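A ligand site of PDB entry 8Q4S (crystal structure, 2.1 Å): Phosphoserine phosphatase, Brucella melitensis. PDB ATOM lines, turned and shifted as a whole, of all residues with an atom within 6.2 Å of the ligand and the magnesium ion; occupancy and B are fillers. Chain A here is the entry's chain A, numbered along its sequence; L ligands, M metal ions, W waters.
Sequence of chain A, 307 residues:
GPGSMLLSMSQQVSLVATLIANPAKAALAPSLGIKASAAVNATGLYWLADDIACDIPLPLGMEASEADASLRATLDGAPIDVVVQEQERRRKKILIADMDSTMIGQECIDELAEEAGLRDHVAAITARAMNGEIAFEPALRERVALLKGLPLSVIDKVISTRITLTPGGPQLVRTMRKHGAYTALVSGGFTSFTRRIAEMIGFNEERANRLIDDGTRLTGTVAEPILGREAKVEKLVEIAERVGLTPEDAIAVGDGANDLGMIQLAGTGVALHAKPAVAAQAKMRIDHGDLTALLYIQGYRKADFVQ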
ATOM      1  N   ASP A  98     -22.882   6.422   2.835  1.00  0.00           N
ATOM      2  CA  ASP A  98     -24.106   5.817   3.305  1.00  0.00           C
ATOM      3  C   ASP A  98     -24.936   6.832   4.100  1.00  0.00           C
ATOM      4  O   ASP A  98     -24.398   7.802   4.636  1.00  0.00           O
ATOM      5  CB  ASP A  98     -23.754   4.626   4.196  1.00  0.00           C
ATOM      6  CG  ASP A  98     -24.963   3.921   4.701  1.00  0.00           C
ATOM      7  OD1 ASP A  98     -25.876   3.749   3.872  1.00  0.00           O
ATOM      8  OD2 ASP A  98     -25.013   3.562   5.895  1.00  0.00           O
ATOM      9  N   MET A  99     -26.259   6.617   4.178  1.00  0.00           N
ATOM     10  CA  MET A  99     -27.105   7.482   5.018  1.00  0.00           C
ATOM     11  C   MET A  99     -27.322   6.914   6.419  1.00  0.00           C
ATOM     12  O   MET A  99     -26.858   7.504   7.401  1.00  0.00           O
ATOM     13  CB  MET A  99     -28.465   7.742   4.363  1.00  0.00           C
ATOM     14  CG  MET A  99     -29.283   8.794   5.144  1.00  0.00           C
ATOM     15  SD  MET A  99     -30.947   9.172   4.527  1.00  0.00           S
ATOM     16  CE  MET A  99     -31.720   7.539   4.597  1.00  0.00           C
ATOM     17  N   ASP A 100     -28.068   5.818   6.532  1.00  0.00           N
ATOM     18  CA  ASP A 100     -28.552   5.343   7.820  1.00  0.00           C
ATOM     19  C   ASP A 100     -27.384   5.022   8.748  1.00  0.00           C
ATOM     20  O   ASP A 100     -26.466   4.286   8.374  1.00  0.00           O
ATOM     21  CB  ASP A 100     -29.421   4.096   7.635  1.00  0.00           C
ATOM     22  CG  ASP A 100     -30.851   4.431   7.166  1.00  0.00           C
ATOM     23  OD1 ASP A 100     -31.342   5.539   7.391  1.00  0.00           O
ATOM     24  OD2 ASP A 100     -31.484   3.566   6.560  1.00  0.00           O
ATOM     25  N   SER A 101     -27.430   5.586   9.948  1.00  0.00           N
ATOM     26  CA  SER A 101     -26.433   5.394  11.006  1.00  0.00           C
ATOM     27  C   SER A 101     -25.086   5.953  10.639  1.00  0.00           C
ATOM     28  O   SER A 101     -24.107   5.711  11.339  1.00  0.00           O
ATOM     29  CB  SER A 101     -26.247   3.910  11.376  1.00  0.00           C
ATOM     30  OG  SER A 101     -27.405   3.444  12.038  1.00  0.00           O
ATOM     31  N   THR A 102     -24.991   6.683   9.521  1.00  0.00           N
ATOM     32  CA  THR A 102     -23.729   7.280   9.101  1.00  0.00           C
ATOM     33  C   THR A 102     -23.904   8.788   9.036  1.00  0.00           C
ATOM     34  O   THR A 102     -23.355   9.481   9.903  1.00  0.00           O
ATOM     35  CB  THR A 102     -23.278   6.665   7.771  1.00  0.00           C
ATOM     36  OG1 THR A 102     -23.074   5.257   7.945  1.00  0.00           O
ATOM     37  CG2 THR A 102     -21.986   7.271   7.266  1.00  0.00           C
ATOM     38  N   GLU A 107     -31.969   4.536  11.800  1.00  0.00           N
ATOM     39  CA  GLU A 107     -32.282   3.659  10.672  1.00  0.00           C
ATOM     40  C   GLU A 107     -33.692   4.034  10.239  1.00  0.00           C
ATOM     41  O   GLU A 107     -34.648   3.812  10.991  1.00  0.00           O
ATOM     42  CB  GLU A 107     -32.211   2.194  11.085  1.00  0.00           C
ATOM     43  CG  GLU A 107     -30.824   1.698  11.512  1.00  0.00           C
ATOM     44  CD  GLU A 107     -29.929   1.441  10.315  1.00  0.00           C
ATOM     45  OE1 GLU A 107     -30.473   1.237   9.210  1.00  0.00           O
ATOM     46  OE2 GLU A 107     -28.699   1.462  10.470  1.00  0.00           O
ATOM     47  N   CYS A 108     -33.812   4.600   9.026  1.00  0.00           N
ATOM     48  CA  CYS A 108     -35.106   5.050   8.531  1.00  0.00           C
ATOM     49  C   CYS A 108     -36.139   3.929   8.558  1.00  0.00           C
ATOM     50  O   CYS A 108     -37.323   4.166   8.860  1.00  0.00           O
ATOM     51  CB  CYS A 108     -34.954   5.643   7.113  1.00  0.00           C
ATOM     52  SG  CYS A 108     -34.281   4.571   5.724  1.00  0.00           S
ATOM     53  N   ILE A 109     -35.708   2.689   8.300  1.00  0.00           N
ATOM     54  CA  ILE A 109     -36.630   1.568   8.254  1.00  0.00           C
ATOM     55  C   ILE A 109     -37.086   1.184   9.661  1.00  0.00           C
ATOM     56  O   ILE A 109     -38.235   0.773   9.851  1.00  0.00           O
ATOM     57  CB  ILE A 109     -36.000   0.370   7.518  1.00  0.00           C
ATOM     58  CG1 ILE A 109     -37.069  -0.678   7.240  1.00  0.00           C
ATOM     59  CG2 ILE A 109     -34.861  -0.252   8.301  1.00  0.00           C
ATOM     60  CD1 ILE A 109     -36.975  -1.210   5.851  1.00  0.00           C
ATOM     61  N   THR A 126     -32.661  -5.566  11.017  1.00  0.00           N
ATOM     62  CA  THR A 126     -31.710  -4.566  10.549  1.00  0.00           C
ATOM     63  C   THR A 126     -30.327  -4.826  11.111  1.00  0.00           C
ATOM     64  O   THR A 126     -29.323  -4.795  10.380  1.00  0.00           O
ATOM     65  CB  THR A 126     -32.191  -3.168  10.946  1.00  0.00           C
ATOM     66  OG1 THR A 126     -33.499  -2.968  10.408  1.00  0.00           O
ATOM     67  CG2 THR A 126     -31.254  -2.117  10.410  1.00  0.00           C
ATOM     68  N   ALA A 129     -28.774  -7.640   9.256  1.00  0.00           N
ATOM     69  CA  ALA A 129     -28.419  -7.255   7.887  1.00  0.00           C
ATOM     70  C   ALA A 129     -27.178  -6.379   7.874  1.00  0.00           C
ATOM     71  O   ALA A 129     -26.276  -6.569   7.048  1.00  0.00           O
ATOM     72  CB  ALA A 129     -29.575  -6.525   7.208  1.00  0.00           C
ATOM     73  N   MET A 130     -27.109  -5.408   8.796  1.00  0.00           N
ATOM     74  CA  MET A 130     -25.947  -4.532   8.791  1.00  0.00           C
ATOM     75  C   MET A 130     -24.698  -5.236   9.287  1.00  0.00           C
ATOM     76  O   MET A 130     -23.596  -4.851   8.911  1.00  0.00           O
ATOM     77  CB  MET A 130     -26.262  -3.268   9.604  1.00  0.00           C
ATOM     78  CG  MET A 130     -27.363  -2.387   8.919  1.00  0.00           C
ATOM     79  SD  MET A 130     -26.931  -1.837   7.215  1.00  0.00           S
ATOM     80  CE  MET A 130     -27.670  -3.125   6.193  1.00  0.00           C
ATOM     81  N   PHE A 136     -28.656  -8.235   1.975  1.00  0.00           N
ATOM     82  CA  PHE A 136     -29.423  -7.003   2.122  1.00  0.00           C
ATOM     83  C   PHE A 136     -30.821  -7.123   1.516  1.00  0.00           C
ATOM     84  O   PHE A 136     -31.817  -6.746   2.146  1.00  0.00           O
ATOM     85  CB  PHE A 136     -28.686  -5.829   1.492  1.00  0.00           C
ATOM     86  CG  PHE A 136     -29.417  -4.543   1.670  1.00  0.00           C
ATOM     87  CD1 PHE A 136     -29.378  -3.890   2.894  1.00  0.00           C
ATOM     88  CD2 PHE A 136     -30.182  -4.017   0.640  1.00  0.00           C
ATOM     89  CE1 PHE A 136     -30.068  -2.705   3.087  1.00  0.00           C
ATOM     90  CE2 PHE A 136     -30.871  -2.823   0.823  1.00  0.00           C
ATOM     91  CZ  PHE A 136     -30.813  -2.165   2.062  1.00  0.00           C
ATOM     92  N   LEU A 140     -34.327  -6.430   3.363  1.00  0.00           N
ATOM     93  CA  LEU A 140     -35.141  -5.259   3.058  1.00  0.00           C
ATOM     94  C   LEU A 140     -36.579  -5.661   2.748  1.00  0.00           C
ATOM     95  O   LEU A 140     -37.525  -5.058   3.268  1.00  0.00           O
ATOM     96  CB  LEU A 140     -34.536  -4.492   1.892  1.00  0.00           C
ATOM     97  CG  LEU A 140     -35.175  -3.158   1.547  1.00  0.00           C
ATOM     98  CD1 LEU A 140     -35.063  -2.181   2.730  1.00  0.00           C
ATOM     99  CD2 LEU A 140     -34.488  -2.598   0.293  1.00  0.00           C
ATOM    100  N   ARG A 143     -38.528  -6.619   5.876  1.00  0.00           N
ATOM    101  CA  ARG A 143     -38.877  -5.507   6.751  1.00  0.00           C
ATOM    102  C   ARG A 143     -39.909  -4.584   6.106  1.00  0.00           C
ATOM    103  O   ARG A 143     -40.849  -4.152   6.758  1.00  0.00           O
ATOM    104  CB  ARG A 143     -37.626  -4.717   7.117  1.00  0.00           C
ATOM    105  CG  ARG A 143     -36.651  -5.512   7.978  1.00  0.00           C
ATOM    106  CD  ARG A 143     -35.328  -4.782   8.114  1.00  0.00           C
ATOM    107  NE  ARG A 143     -34.520  -4.831   6.899  1.00  0.00           N
ATOM    108  CZ  ARG A 143     -33.452  -4.074   6.692  1.00  0.00           C
ATOM    109  NH1 ARG A 143     -33.058  -3.183   7.588  1.00  0.00           N
ATOM    110  NH2 ARG A 143     -32.761  -4.195   5.561  1.00  0.00           N
ATOM    111  N   VAL A 186     -25.503   7.774  -1.000  1.00  0.00           N
ATOM    112  CA  VAL A 186     -25.905   6.557  -1.677  1.00  0.00           C
ATOM    113  C   VAL A 186     -26.294   5.536  -0.617  1.00  0.00           C
ATOM    114  O   VAL A 186     -25.451   5.100   0.173  1.00  0.00           O
ATOM    115  CB  VAL A 186     -24.783   6.037  -2.601  1.00  0.00           C
ATOM    116  CG1 VAL A 186     -25.197   4.766  -3.306  1.00  0.00           C
ATOM    117  CG2 VAL A 186     -24.408   7.122  -3.623  1.00  0.00           C
ATOM    118  N   SER A 187     -27.569   5.139  -0.624  1.00  0.00           N
ATOM    119  CA  SER A 187     -28.213   4.527   0.527  1.00  0.00           C
ATOM    120  C   SER A 187     -29.056   3.317   0.120  1.00  0.00           C
ATOM    121  O   SER A 187     -29.687   3.326  -0.948  1.00  0.00           O
ATOM    122  CB  SER A 187     -29.089   5.583   1.244  1.00  0.00           C
ATOM    123  OG  SER A 187     -29.957   5.017   2.213  1.00  0.00           O
ATOM    124  N   GLY A 188     -29.065   2.288   0.966  1.00  0.00           N
ATOM    125  CA  GLY A 188     -30.035   1.227   0.811  1.00  0.00           C
ATOM    126  C   GLY A 188     -31.404   1.598   1.322  1.00  0.00           C
ATOM    127  O   GLY A 188     -32.326   0.778   1.250  1.00  0.00           O
ATOM    128  N   GLY A 189     -31.566   2.819   1.854  1.00  0.00           N
ATOM    129  CA  GLY A 189     -32.833   3.290   2.362  1.00  0.00           C
ATOM    130  C   GLY A 189     -33.693   3.854   1.251  1.00  0.00           C
ATOM    131  O   GLY A 189     -33.620   3.405   0.107  1.00  0.00           O
ATOM    132  N   PHE A 190     -34.486   4.881   1.575  1.00  0.00           N
ATOM    133  CA  PHE A 190     -35.577   5.298   0.706  1.00  0.00           C
ATOM    134  C   PHE A 190     -35.412   6.733   0.216  1.00  0.00           C
ATOM    135  O   PHE A 190     -35.012   7.634   0.961  1.00  0.00           O
ATOM    136  CB  PHE A 190     -36.897   5.112   1.433  1.00  0.00           C
ATOM    137  CG  PHE A 190     -37.013   3.741   2.066  1.00  0.00           C
ATOM    138  CD1 PHE A 190     -36.960   2.596   1.277  1.00  0.00           C
ATOM    139  CD2 PHE A 190     -37.106   3.597   3.440  1.00  0.00           C
ATOM    140  CE1 PHE A 190     -37.039   1.320   1.834  1.00  0.00           C
ATOM    141  CE2 PHE A 190     -37.183   2.333   4.018  1.00  0.00           C
ATOM    142  CZ  PHE A 190     -37.146   1.193   3.214  1.00  0.00           C
ATOM    143  N   THR A 194     -33.789  10.199   1.608  1.00  0.00           N
ATOM    144  CA  THR A 194     -32.490  10.710   1.141  1.00  0.00           C
ATOM    145  C   THR A 194     -32.625  12.053   0.429  1.00  0.00           C
ATOM    146  O   THR A 194     -31.717  12.880   0.517  1.00  0.00           O
ATOM    147  CB  THR A 194     -31.814   9.725   0.179  1.00  0.00           C
ATOM    148  OG1 THR A 194     -32.711   9.416  -0.904  1.00  0.00           O
ATOM    149  CG2 THR A 194     -31.389   8.450   0.902  1.00  0.00           C
ATOM    150  N   LYS A 232     -23.979  -0.177  -4.687  1.00  0.00           N
ATOM    151  CA  LYS A 232     -23.138   0.920  -4.238  1.00  0.00           C
ATOM    152  C   LYS A 232     -21.808   0.937  -4.983  1.00  0.00           C
ATOM    153  O   LYS A 232     -21.302   1.999  -5.350  1.00  0.00           O
ATOM    154  CB  LYS A 232     -22.921   0.844  -2.711  1.00  0.00           C
ATOM    155  CG  LYS A 232     -24.232   0.937  -1.896  1.00  0.00           C
ATOM    156  CD  LYS A 232     -24.014   1.470  -0.452  1.00  0.00           C
ATOM    157  CE  LYS A 232     -25.271   1.308   0.413  1.00  0.00           C
ATOM    158  NZ  LYS A 232     -25.380   2.359   1.476  1.00  0.00           N
ATOM    159  N   GLY A 254     -19.115   4.206   5.422  1.00  0.00           N
ATOM    160  CA  GLY A 254     -20.359   3.644   5.911  1.00  0.00           C
ATOM    161  C   GLY A 254     -20.105   2.845   7.176  1.00  0.00           C
ATOM    162  O   GLY A 254     -18.990   2.774   7.691  1.00  0.00           O
ATOM    163  N   ASP A 255     -21.181   2.259   7.677  1.00  0.00           N
ATOM    164  CA  ASP A 255     -21.174   1.468   8.894  1.00  0.00           C
ATOM    165  C   ASP A 255     -21.560   0.022   8.687  1.00  0.00           C
ATOM    166  O   ASP A 255     -21.316  -0.799   9.583  1.00  0.00           O
ATOM    167  CB  ASP A 255     -22.151   2.072   9.916  1.00  0.00           C
ATOM    168  CG  ASP A 255     -23.612   1.902   9.481  1.00  0.00           C
ATOM    169  OD1 ASP A 255     -23.962   2.335   8.371  1.00  0.00           O
ATOM    170  OD2 ASP A 255     -24.398   1.307  10.237  1.00  0.00           O
ATOM    171  N   GLY A 256     -22.161  -0.327   7.547  1.00  0.00           N
ATOM    172  CA  GLY A 256     -22.839  -1.602   7.409  1.00  0.00           C
ATOM    173  C   GLY A 256     -22.178  -2.514   6.379  1.00  0.00           C
ATOM    174  O   GLY A 256     -21.334  -2.112   5.576  1.00  0.00           O
ATOM    175  N   ASN A 258     -23.459  -3.786   3.777  1.00  0.00           N
ATOM    176  CA  ASN A 258     -23.765  -3.381   2.416  1.00  0.00           C
ATOM    177  C   ASN A 258     -22.884  -2.227   1.913  1.00  0.00           C
ATOM    178  O   ASN A 258     -23.014  -1.847   0.743  1.00  0.00           O
ATOM    179  CB  ASN A 258     -25.236  -3.007   2.283  1.00  0.00           C
ATOM    180  CG  ASN A 258     -25.643  -1.896   3.223  1.00  0.00           C
ATOM    181  OD1 ASN A 258     -25.148  -1.798   4.354  1.00  0.00           O
ATOM    182  ND2 ASN A 258     -26.550  -1.032   2.765  1.00  0.00           N
ATOM    183  N   ASP A 259     -21.980  -1.684   2.732  1.00  0.00           N
ATOM    184  CA  ASP A 259     -21.073  -0.617   2.313  1.00  0.00           C
ATOM    185  C   ASP A 259     -19.683  -1.133   2.004  1.00  0.00           C
ATOM    186  O   ASP A 259     -18.854  -0.359   1.513  1.00  0.00           O
ATOM    187  CB  ASP A 259     -20.939   0.468   3.395  1.00  0.00           C
ATOM    188  CG  ASP A 259     -22.264   1.085   3.756  1.00  0.00           C
ATOM    189  OD1 ASP A 259     -23.005   1.416   2.810  1.00  0.00           O
ATOM    190  OD2 ASP A 259     -22.577   1.237   4.962  1.00  0.00           O
ATOM    191  N   LYS A 275     -20.465  -1.874  12.519  1.00  0.00           N
ATOM    192  CA  LYS A 275     -20.830  -3.149  13.118  1.00  0.00           C
ATOM    193  C   LYS A 275     -19.569  -3.993  13.319  1.00  0.00           C
ATOM    194  O   LYS A 275     -18.565  -3.819  12.601  1.00  0.00           O
ATOM    195  CB  LYS A 275     -21.887  -3.832  12.246  1.00  0.00           C
ATOM    196  CG  LYS A 275     -23.335  -3.381  12.543  1.00  0.00           C
ATOM    197  CD  LYS A 275     -23.538  -1.891  12.243  1.00  0.00           C
ATOM    198  CE  LYS A 275     -24.929  -1.386  12.627  1.00  0.00           C
ATOM    199  NZ  LYS A 275     -24.981   0.129  12.666  1.00  0.00           N
HETATM  200  O1  LIG L   1     -27.646   2.342   5.678  1.00  0.00           O
HETATM  201  O2  LIG L   1     -28.421   4.142   4.134  1.00  0.00           O
HETATM  202  C1  LIG L   1     -30.157   2.047   4.517  1.00  0.00           C
HETATM  203  C2  LIG L   1     -31.138  -1.184   6.208  1.00  0.00           C
HETATM  204  C3  LIG L   1     -30.555   0.231   6.204  1.00  0.00           C
HETATM  205  C4  LIG L   1     -30.196   0.552   4.767  1.00  0.00           C
HETATM  206  O3  LIG L   1     -30.652  -2.093   6.927  1.00  0.00           O
HETATM  207  O4  LIG L   1     -32.110  -1.461   5.473  1.00  0.00           O
HETATM  208  N1  LIG L   1     -29.360   0.322   7.045  1.00  0.00           N
HETATM  209  P1  LIG L   1     -28.398   2.632   4.383  1.00  0.00           P
HETATM  210  O5  LIG L   1     -27.729   1.827   3.278  1.00  0.00           O
HETATM  211 MG    MG M   1     -25.827   2.394   7.173  1.00  0.00          MG
HETATM  212  O   HOH W   1     -33.439   0.509   4.596  1.00  0.00           O
HETATM  213  O   HOH W   2     -24.973   0.644   5.725  1.00  0.00           O
HETATM  214  O   HOH W   3     -26.784   1.019   8.754  1.00  0.00           O
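The backbone NH (N) of Asp 100 is in hydrogen-bond range of an oxygen (O2) of the ligand (2.9 Å). The side-chain carboxylate (OD2) of Asp 100 is in salt-bridge range of a nitrogen (N1) of the ligand, at 3.9 Å. OE1 of Glu 107 lies within salt-bridge range of N1 of the ligand, 2.6 Å away. The side-chain hydroxyl of Ser 187 sits at hydrogen-bond distance from an oxygen (O2) of the ligand (2.6 Å). An oxygen (O5) of the ligand lies within hydrogen-bond range of the backbone NH (N) of Gly 188, at 2.7 Å. The guanidinium group (NH1) of Arg 143 lies within salt-bridge range of an oxygen (O3) of the ligand (2.7 Å). The side-chain amino group (NZ) of Lys 232 lies within salt-bridge range of an oxygen (O5) of the ligand (3.0 Å). O5 of the ligand lies within hydrogen-bond range of ND2 of Asn 258. The side-chain sulfur of Met 130 sits at hydrogen-bond distance from a nitrogen (N1) of the ligand, 3.3 Å away. An oxygen (O2) of the ligand sits at hydrogen-bond distance from the backbone NH (N) of Met 99, at 3.3 Å.
OD2 of Asp 98 sits close to OG1 of Thr 102. The side-chain carboxylate (OD1) of Asp 255 sits close to the side-chain hydroxyl (OG1) of Thr 102 (3.1 Å). The side-chain carboxylate (OD2) of Asp 259 lies within hydrogen-bond range of the backbone NH (N) of Asp 255 (3.2 Å). The side-chain carboxylate (OD2) of Asp 100 is in hydrogen-bond range of the side-chain sulfur (SG) of Cys 108 (3.1 Å). The side-chain hydroxyl of Ser 101 is in hydrogen-bond range of the side-chain carboxylate of Glu 107 (2.8 Å). The side-chain hydroxyl of Ser 187 sits at hydrogen-bond distance from the backbone NH of Gly 189 (2.7 Å). The side-chain hydroxyl (OG1) of Thr 126 is in hydrogen-bond range of the guanidinium group (NH1) of Arg 143 (2.9 Å). OD1 of Asn 258 lies close to SD of Met 130 (3.4 Å).
Residues that only touch the ligand: Gly 189, Phe 136 and Thr 126. Hydrophobic or aromatic side chains that line the ligand: Met 99, Met 130 and Phe 136. Within 4 Å of the ligand: Asp 98, Met 99, Asp 100, Glu 107, Thr 126, Met 130, Phe 136, Arg 143, Ser 187, Gly 188, Gly 189, Lys 232 and Asn 258.
Within 4 Å of the magnesium ion: Asp 98, Asp 100 and Asp 255. The nearest printed residue that does not touch the magnesium ion is Thr 102 (4.05 Å).
The magnesium ion is bound by the side-chain carboxylate of Asp 98 (1.9 Å), the side-chain carboxylate of Asp 255 (2.2 Å), water W3 (2.3 Å), the backbone carbonyl oxygen of Asp 100 (2.3 Å), an oxygen (O1) of the ligand (2.4 Å) and water W2 (2.4 Å).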
